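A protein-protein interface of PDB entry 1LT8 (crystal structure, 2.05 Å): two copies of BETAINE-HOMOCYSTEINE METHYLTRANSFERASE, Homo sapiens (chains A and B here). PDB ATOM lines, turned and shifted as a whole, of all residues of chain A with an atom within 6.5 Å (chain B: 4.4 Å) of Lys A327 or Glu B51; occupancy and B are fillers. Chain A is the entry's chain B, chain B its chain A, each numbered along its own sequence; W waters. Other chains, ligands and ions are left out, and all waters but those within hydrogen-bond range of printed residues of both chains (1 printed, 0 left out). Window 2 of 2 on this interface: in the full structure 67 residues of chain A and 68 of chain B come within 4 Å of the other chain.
Of the printed residues of chain B, Arg A65 touches Gly B37 (2.7 Å), Tyr B38 (3.5 Å) and His B52 (3.5 Å).
Of the printed residues of chain A, Lys B40 touches Lys A327 and His A328.
Of the printed residues of chain A, His B52 touches Arg A65 (3.5 Å).
The nearest residue of chain A that does not touch Glu B51 is Arg A65 (5.5 Å).
The nearest printed residue of chain A that does not touch Glu B47 is Glu A326 (6.5 Å).
Of the 11 printed residues of chain B, 7 touch a printed residue of chain A.
Printed residues of chain B that touch a printed residue of chain A: Gly B37, Tyr B38, Val B39, Lys B40, Glu B47, Glu B51 and His B52.
Along chain B the printed residues that touch a printed residue of chain A span positions 37 to 52.
Among the printed residues, 11 pairs touch across the chains.
Among the printed residues, Asp or Glu carboxylates within 4 Å of a Lys or Arg side-chain nitrogen of the other chain: Lys A327 with Glu B47 (2.6 Å) and Lys A327 with Glu B51 (2.8 Å).
Among the printed residues, merely in contact across the chains: Arg A65 with Tyr B38, Lys A327 with Gly B37, Lys A327 with Lys B40, Lys A327 with Tyr B38 and Arg A308 with Gly B37.
The backbone carbonyl oxygen (O) of Ala A324 is in hydrogen-bond range of the guanidinium group (NH2) of Arg A308.
The side-chain carboxylate (OE1) of Glu A312 is in salt-bridge range of the guanidinium group (NE) of Arg A308 (3.96 Å).
The backbone NH of Ala A324 is in hydrogen-bond range of the backbone carbonyl oxygen of Arg A65 (3.0 Å).
OE2 of Glu A312 sits at hydrogen-bond distance from ND1 of His A328 (2.9 Å).
NH2 of Arg A308 sits at hydrogen-bond distance from O of Lys A327.
NH2 of Arg A278 is in hydrogen-bond range of NE2 of His A328 (3.0 Å).
NZ of Lys A327 lies within salt-bridge range of OE1 of Glu B47.
The side-chain carboxylate of Glu B51 is in salt-bridge range of the side-chain amino group of Lys A327 (2.8 Å).
O of Lys A327 lies close to O of Val B39, at 3.1 Å.
A ring nitrogen (NE2) of His B52 is in hydrogen-bond range of the guanidinium group of Arg A65 (3.5 Å).
O of His A328 lies within hydrogen-bond range of NZ of Lys B40, 3.3 Å away.
NE of Arg A65 sits at hydrogen-bond distance from O of Gly B37 (2.7 Å).
Water W1 lies within hydrogen-bond range of the guanidinium group of Arg A308 (2.4 Å), the backbone carbonyl oxygen of Val B39 (2.7 Å) and the backbone carbonyl oxygen of Lys A327 (3.1 Å).
No position is printed for both chains.
Of the 11 pairs that touch across the chains among the printed residues, none has its exchanged pair printed and touching as well.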
ATOM      1  N   ARG A  65      14.141 -16.006  14.770  1.00  0.00           N
ATOM      2  CA  ARG A  65      14.197 -15.568  13.377  1.00  0.00           C
ATOM      3  C   ARG A  65      13.719 -16.670  12.430  1.00  0.00           C
ATOM      4  O   ARG A  65      13.219 -16.387  11.344  1.00  0.00           O
ATOM      5  CB  ARG A  65      15.631 -15.170  13.027  1.00  0.00           C
ATOM      6  CG  ARG A  65      15.843 -14.777  11.568  1.00  0.00           C
ATOM      7  CD  ARG A  65      17.309 -14.605  11.268  1.00  0.00           C
ATOM      8  NE  ARG A  65      17.549 -14.254   9.871  1.00  0.00           N
ATOM      9  CZ  ARG A  65      17.239 -13.081   9.321  1.00  0.00           C
ATOM     10  NH1 ARG A  65      16.668 -12.126  10.048  1.00  0.00           N
ATOM     11  NH2 ARG A  65      17.504 -12.859   8.041  1.00  0.00           N
ATOM     12  N   ARG A 278      16.206 -30.247   5.426  1.00  0.00           N
ATOM     13  CA  ARG A 278      15.080 -29.362   5.656  1.00  0.00           C
ATOM     14  C   ARG A 278      13.827 -29.975   5.034  1.00  0.00           C
ATOM     15  O   ARG A 278      12.721 -29.749   5.516  1.00  0.00           O
ATOM     16  CB  ARG A 278      15.351 -27.978   5.066  1.00  0.00           C
ATOM     17  CG  ARG A 278      15.586 -27.936   3.566  1.00  0.00           C
ATOM     18  CD  ARG A 278      16.264 -26.626   3.221  1.00  0.00           C
ATOM     19  NE  ARG A 278      17.642 -26.613   3.716  1.00  0.00           N
ATOM     20  CZ  ARG A 278      18.407 -25.529   3.795  1.00  0.00           C
ATOM     21  NH1 ARG A 278      19.650 -25.627   4.252  1.00  0.00           N
ATOM     22  NH2 ARG A 278      17.932 -24.344   3.439  1.00  0.00           N
ATOM     23  N   ARG A 308      12.836 -23.389  10.705  1.00  0.00           N
ATOM     24  CA  ARG A 308      12.363 -22.611   9.576  1.00  0.00           C
ATOM     25  C   ARG A 308      11.592 -23.483   8.575  1.00  0.00           C
ATOM     26  O   ARG A 308      10.627 -23.028   7.952  1.00  0.00           O
ATOM     27  CB  ARG A 308      13.547 -21.951   8.887  1.00  0.00           C
ATOM     28  CG  ARG A 308      13.192 -21.366   7.559  1.00  0.00           C
ATOM     29  CD  ARG A 308      14.314 -21.603   6.565  1.00  0.00           C
ATOM     30  NE  ARG A 308      15.187 -20.451   6.425  1.00  0.00           N
ATOM     31  CZ  ARG A 308      16.405 -20.498   5.897  1.00  0.00           C
ATOM     32  NH1 ARG A 308      16.915 -21.649   5.465  1.00  0.00           N
ATOM     33  NH2 ARG A 308      17.099 -19.385   5.778  1.00  0.00           N
ATOM     34  N   GLU A 312       8.013 -22.707   7.051  1.00  0.00           N
ATOM     35  CA  GLU A 312       7.790 -22.553   5.617  1.00  0.00           C
ATOM     36  C   GLU A 312       6.782 -23.557   5.092  1.00  0.00           C
ATOM     37  O   GLU A 312       5.920 -23.215   4.285  1.00  0.00           O
ATOM     38  CB  GLU A 312       9.109 -22.686   4.847  1.00  0.00           C
ATOM     39  CG  GLU A 312      10.070 -21.530   5.094  1.00  0.00           C
ATOM     40  CD  GLU A 312      11.308 -21.599   4.215  1.00  0.00           C
ATOM     41  OE1 GLU A 312      11.998 -20.569   4.083  1.00  0.00           O
ATOM     42  OE2 GLU A 312      11.588 -22.683   3.664  1.00  0.00           O
ATOM     43  N   PRO A 323      11.153 -14.325   9.335  1.00  0.00           N
ATOM     44  CA  PRO A 323      12.203 -13.410   8.878  1.00  0.00           C
ATOM     45  C   PRO A 323      13.321 -14.133   8.121  1.00  0.00           C
ATOM     46  O   PRO A 323      13.845 -13.627   7.127  1.00  0.00           O
ATOM     47  CB  PRO A 323      12.713 -12.802  10.182  1.00  0.00           C
ATOM     48  CG  PRO A 323      11.521 -12.818  11.051  1.00  0.00           C
ATOM     49  CD  PRO A 323      10.923 -14.169  10.781  1.00  0.00           C
ATOM     50  N   ALA A 324      13.690 -15.312   8.608  1.00  0.00           N
ATOM     51  CA  ALA A 324      14.753 -16.091   7.987  1.00  0.00           C
ATOM     52  C   ALA A 324      14.436 -16.525   6.560  1.00  0.00           C
ATOM     53  O   ALA A 324      15.331 -16.957   5.835  1.00  0.00           O
ATOM     54  CB  ALA A 324      15.065 -17.312   8.839  1.00  0.00           C
ATOM     55  N   SER A 325      13.173 -16.416   6.153  1.00  0.00           N
ATOM     56  CA  SER A 325      12.784 -16.812   4.801  1.00  0.00           C
ATOM     57  C   SER A 325      13.231 -15.826   3.745  1.00  0.00           C
ATOM     58  O   SER A 325      13.150 -16.109   2.549  1.00  0.00           O
ATOM     59  CB  SER A 325      11.275 -17.016   4.707  1.00  0.00           C
ATOM     60  OG  SER A 325      10.899 -18.219   5.353  1.00  0.00           O
ATOM     61  N   GLU A 326      13.698 -14.664   4.185  1.00  0.00           N
ATOM     62  CA  GLU A 326      14.182 -13.664   3.245  1.00  0.00           C
ATOM     63  C   GLU A 326      15.538 -14.153   2.744  1.00  0.00           C
ATOM     64  O   GLU A 326      16.068 -13.645   1.757  1.00  0.00           O
ATOM     65  CB  GLU A 326      14.338 -12.304   3.931  1.00  0.00           C
ATOM     66  CG  GLU A 326      14.727 -11.183   2.974  1.00  0.00           C
ATOM     67  CD  GLU A 326      13.648 -10.870   1.939  1.00  0.00           C
ATOM     68  OE1 GLU A 326      13.929 -10.065   1.021  1.00  0.00           O
ATOM     69  OE2 GLU A 326      12.524 -11.418   2.049  1.00  0.00           O
ATOM     70  N   LYS A 327      16.088 -15.148   3.437  1.00  0.00           N
ATOM     71  CA  LYS A 327      17.381 -15.729   3.080  1.00  0.00           C
ATOM     72  C   LYS A 327      17.208 -17.172   2.617  1.00  0.00           C
ATOM     73  O   LYS A 327      18.039 -18.032   2.907  1.00  0.00           O
ATOM     74  CB  LYS A 327      18.331 -15.696   4.284  1.00  0.00           C
ATOM     75  CG  LYS A 327      18.606 -14.305   4.833  1.00  0.00           C
ATOM     76  CD  LYS A 327      19.244 -13.402   3.788  1.00  0.00           C
ATOM     77  CE  LYS A 327      19.441 -11.997   4.335  1.00  0.00           C
ATOM     78  NZ  LYS A 327      20.120 -11.090   3.361  1.00  0.00           N
ATOM     79  N   HIS A 328      16.122 -17.437   1.900  1.00  0.00           N
ATOM     80  CA  HIS A 328      15.854 -18.784   1.409  1.00  0.00           C
ATOM     81  C   HIS A 328      14.999 -18.692   0.151  1.00  0.00           C
ATOM     82  O   HIS A 328      14.814 -17.612  -0.415  1.00  0.00           O
ATOM     83  CB  HIS A 328      15.115 -19.603   2.483  1.00  0.00           C
ATOM     84  CG  HIS A 328      15.185 -21.091   2.284  1.00  0.00           C
ATOM     85  ND1 HIS A 328      14.271 -21.958   2.842  1.00  0.00           N
ATOM     86  CD2 HIS A 328      16.078 -21.864   1.616  1.00  0.00           C
ATOM     87  CE1 HIS A 328      14.595 -23.202   2.529  1.00  0.00           C
ATOM     88  NE2 HIS A 328      15.688 -23.173   1.788  1.00  0.00           N
ATOM     89  N   GLY A 329      14.492 -19.841  -0.281  1.00  0.00           N
ATOM     90  CA  GLY A 329      13.639 -19.914  -1.451  1.00  0.00           C
ATOM     91  C   GLY A 329      12.723 -21.104  -1.252  1.00  0.00           C
ATOM     92  O   GLY A 329      13.102 -22.061  -0.577  1.00  0.00           O
ATOM     93  N   GLY B  37      20.264 -18.969   9.262  1.00  0.00           N
ATOM     94  CA  GLY B  37      19.307 -18.006   8.730  1.00  0.00           C
ATOM     95  C   GLY B  37      19.776 -16.635   8.268  1.00  0.00           C
ATOM     96  O   GLY B  37      18.952 -15.736   8.083  1.00  0.00           O
ATOM     97  N   TYR B  38      21.073 -16.463   8.046  1.00  0.00           N
ATOM     98  CA  TYR B  38      21.591 -15.161   7.636  1.00  0.00           C
ATOM     99  C   TYR B  38      22.160 -15.092   6.225  1.00  0.00           C
ATOM    100  O   TYR B  38      22.513 -14.014   5.753  1.00  0.00           O
ATOM    101  CB  TYR B  38      22.642 -14.699   8.652  1.00  0.00           C
ATOM    102  CG  TYR B  38      22.082 -14.621  10.045  1.00  0.00           C
ATOM    103  CD1 TYR B  38      21.231 -13.576  10.417  1.00  0.00           C
ATOM    104  CD2 TYR B  38      22.320 -15.641  10.968  1.00  0.00           C
ATOM    105  CE1 TYR B  38      20.623 -13.555  11.671  1.00  0.00           C
ATOM    106  CE2 TYR B  38      21.719 -15.634  12.223  1.00  0.00           C
ATOM    107  CZ  TYR B  38      20.867 -14.587  12.568  1.00  0.00           C
ATOM    108  OH  TYR B  38      20.248 -14.589  13.803  1.00  0.00           O
ATOM    109  N   VAL B  39      22.241 -16.234   5.549  1.00  0.00           N
ATOM    110  CA  VAL B  39      22.775 -16.271   4.189  1.00  0.00           C
ATOM    111  C   VAL B  39      21.816 -16.985   3.245  1.00  0.00           C
ATOM    112  O   VAL B  39      21.098 -17.904   3.644  1.00  0.00           O
ATOM    113  CB  VAL B  39      24.159 -16.975   4.152  1.00  0.00           C
ATOM    114  CG1 VAL B  39      24.582 -17.254   2.717  1.00  0.00           C
ATOM    115  CG2 VAL B  39      25.196 -16.098   4.822  1.00  0.00           C
ATOM    116  N   LYS B  40      21.814 -16.557   1.988  1.00  0.00           N
ATOM    117  CA  LYS B  40      20.941 -17.131   0.978  1.00  0.00           C
ATOM    118  C   LYS B  40      21.700 -18.059   0.036  1.00  0.00           C
ATOM    119  O   LYS B  40      22.542 -17.611  -0.741  1.00  0.00           O
ATOM    120  CB  LYS B  40      20.282 -16.001   0.182  1.00  0.00           C
ATOM    121  CG  LYS B  40      19.378 -16.447  -0.956  1.00  0.00           C
ATOM    122  CD  LYS B  40      18.773 -15.220  -1.641  1.00  0.00           C
ATOM    123  CE  LYS B  40      18.019 -15.566  -2.920  1.00  0.00           C
ATOM    124  NZ  LYS B  40      16.881 -16.494  -2.681  1.00  0.00           N
ATOM    125  N   GLU B  47      26.054 -10.197   2.834  1.00  0.00           N
ATOM    126  CA  GLU B  47      25.453  -8.963   3.340  1.00  0.00           C
ATOM    127  C   GLU B  47      25.155  -8.971   4.841  1.00  0.00           C
ATOM    128  O   GLU B  47      24.921  -7.915   5.430  1.00  0.00           O
ATOM    129  CB  GLU B  47      24.174  -8.610   2.570  1.00  0.00           C
ATOM    130  CG  GLU B  47      23.017  -9.573   2.744  1.00  0.00           C
ATOM    131  CD  GLU B  47      23.116 -10.766   1.830  1.00  0.00           C
ATOM    132  OE1 GLU B  47      22.209 -11.621   1.880  1.00  0.00           O
ATOM    133  OE2 GLU B  47      24.096 -10.849   1.061  1.00  0.00           O
ATOM    134  N   ALA B  48      25.172 -10.152   5.455  1.00  0.00           N
ATOM    135  CA  ALA B  48      24.900 -10.281   6.886  1.00  0.00           C
ATOM    136  C   ALA B  48      25.869  -9.472   7.737  1.00  0.00           C
ATOM    137  O   ALA B  48      25.562  -9.125   8.876  1.00  0.00           O
ATOM    138  CB  ALA B  48      24.947 -11.749   7.305  1.00  0.00           C
ATOM    139  N   ALA B  49      27.044  -9.182   7.191  1.00  0.00           N
ATOM    140  CA  ALA B  49      28.041  -8.407   7.916  1.00  0.00           C
ATOM    141  C   ALA B  49      27.435  -7.086   8.390  1.00  0.00           C
ATOM    142  O   ALA B  49      27.704  -6.627   9.500  1.00  0.00           O
ATOM    143  CB  ALA B  49      29.231  -8.136   7.023  1.00  0.00           C
ATOM    144  N   VAL B  50      26.615  -6.482   7.534  1.00  0.00           N
ATOM    145  CA  VAL B  50      25.965  -5.216   7.848  1.00  0.00           C
ATOM    146  C   VAL B  50      24.539  -5.403   8.348  1.00  0.00           C
ATOM    147  O   VAL B  50      24.102  -4.712   9.265  1.00  0.00           O
ATOM    148  CB  VAL B  50      25.953  -4.292   6.620  1.00  0.00           C
ATOM    149  CG1 VAL B  50      27.296  -3.603   6.488  1.00  0.00           C
ATOM    150  CG2 VAL B  50      25.672  -5.102   5.374  1.00  0.00           C
ATOM    151  N   GLU B  51      23.814  -6.337   7.745  1.00  0.00           N
ATOM    152  CA  GLU B  51      22.443  -6.607   8.159  1.00  0.00           C
ATOM    153  C   GLU B  51      22.398  -7.203   9.563  1.00  0.00           C
ATOM    154  O   GLU B  51      21.598  -6.781  10.393  1.00  0.00           O
ATOM    155  CB  GLU B  51      21.775  -7.571   7.174  1.00  0.00           C
ATOM    156  CG  GLU B  51      21.247  -6.925   5.901  1.00  0.00           C
ATOM    157  CD  GLU B  51      20.843  -7.954   4.846  1.00  0.00           C
ATOM    158  OE1 GLU B  51      20.303  -9.017   5.225  1.00  0.00           O
ATOM    159  OE2 GLU B  51      21.054  -7.692   3.641  1.00  0.00           O
ATOM    160  N   HIS B  52      23.262  -8.180   9.827  1.00  0.00           N
ATOM    161  CA  HIS B  52      23.291  -8.842  11.133  1.00  0.00           C
ATOM    162  C   HIS B  52      24.711  -9.159  11.604  1.00  0.00           C
ATOM    163  O   HIS B  52      25.150 -10.307  11.541  1.00  0.00           O
ATOM    164  CB  HIS B  52      22.485 -10.144  11.066  1.00  0.00           C
ATOM    165  CG  HIS B  52      21.050  -9.950  10.682  1.00  0.00           C
ATOM    166  ND1 HIS B  52      20.056  -9.734  11.608  1.00  0.00           N
ATOM    167  CD2 HIS B  52      20.450  -9.920   9.469  1.00  0.00           C
ATOM    168  CE1 HIS B  52      18.901  -9.581  10.984  1.00  0.00           C
ATOM    169  NE2 HIS B  52      19.113  -9.688   9.685  1.00  0.00           N
ATOM    170  N   PRO B  53      25.439  -8.146  12.101  1.00  0.00           N
ATOM    171  CA  PRO B  53      26.814  -8.313  12.582  1.00  0.00           C
ATOM    172  C   PRO B  53      26.982  -9.247  13.783  1.00  0.00           C
ATOM    173  O   PRO B  53      27.976  -9.963  13.873  1.00  0.00           O
ATOM    174  CB  PRO B  53      27.245  -6.876  12.884  1.00  0.00           C
ATOM    175  CG  PRO B  53      25.971  -6.240  13.313  1.00  0.00           C
ATOM    176  CD  PRO B  53      24.999  -6.750  12.276  1.00  0.00           C
HETATM  177  O   HOH W   1      19.454 -19.008   5.462  1.00  0.00           O
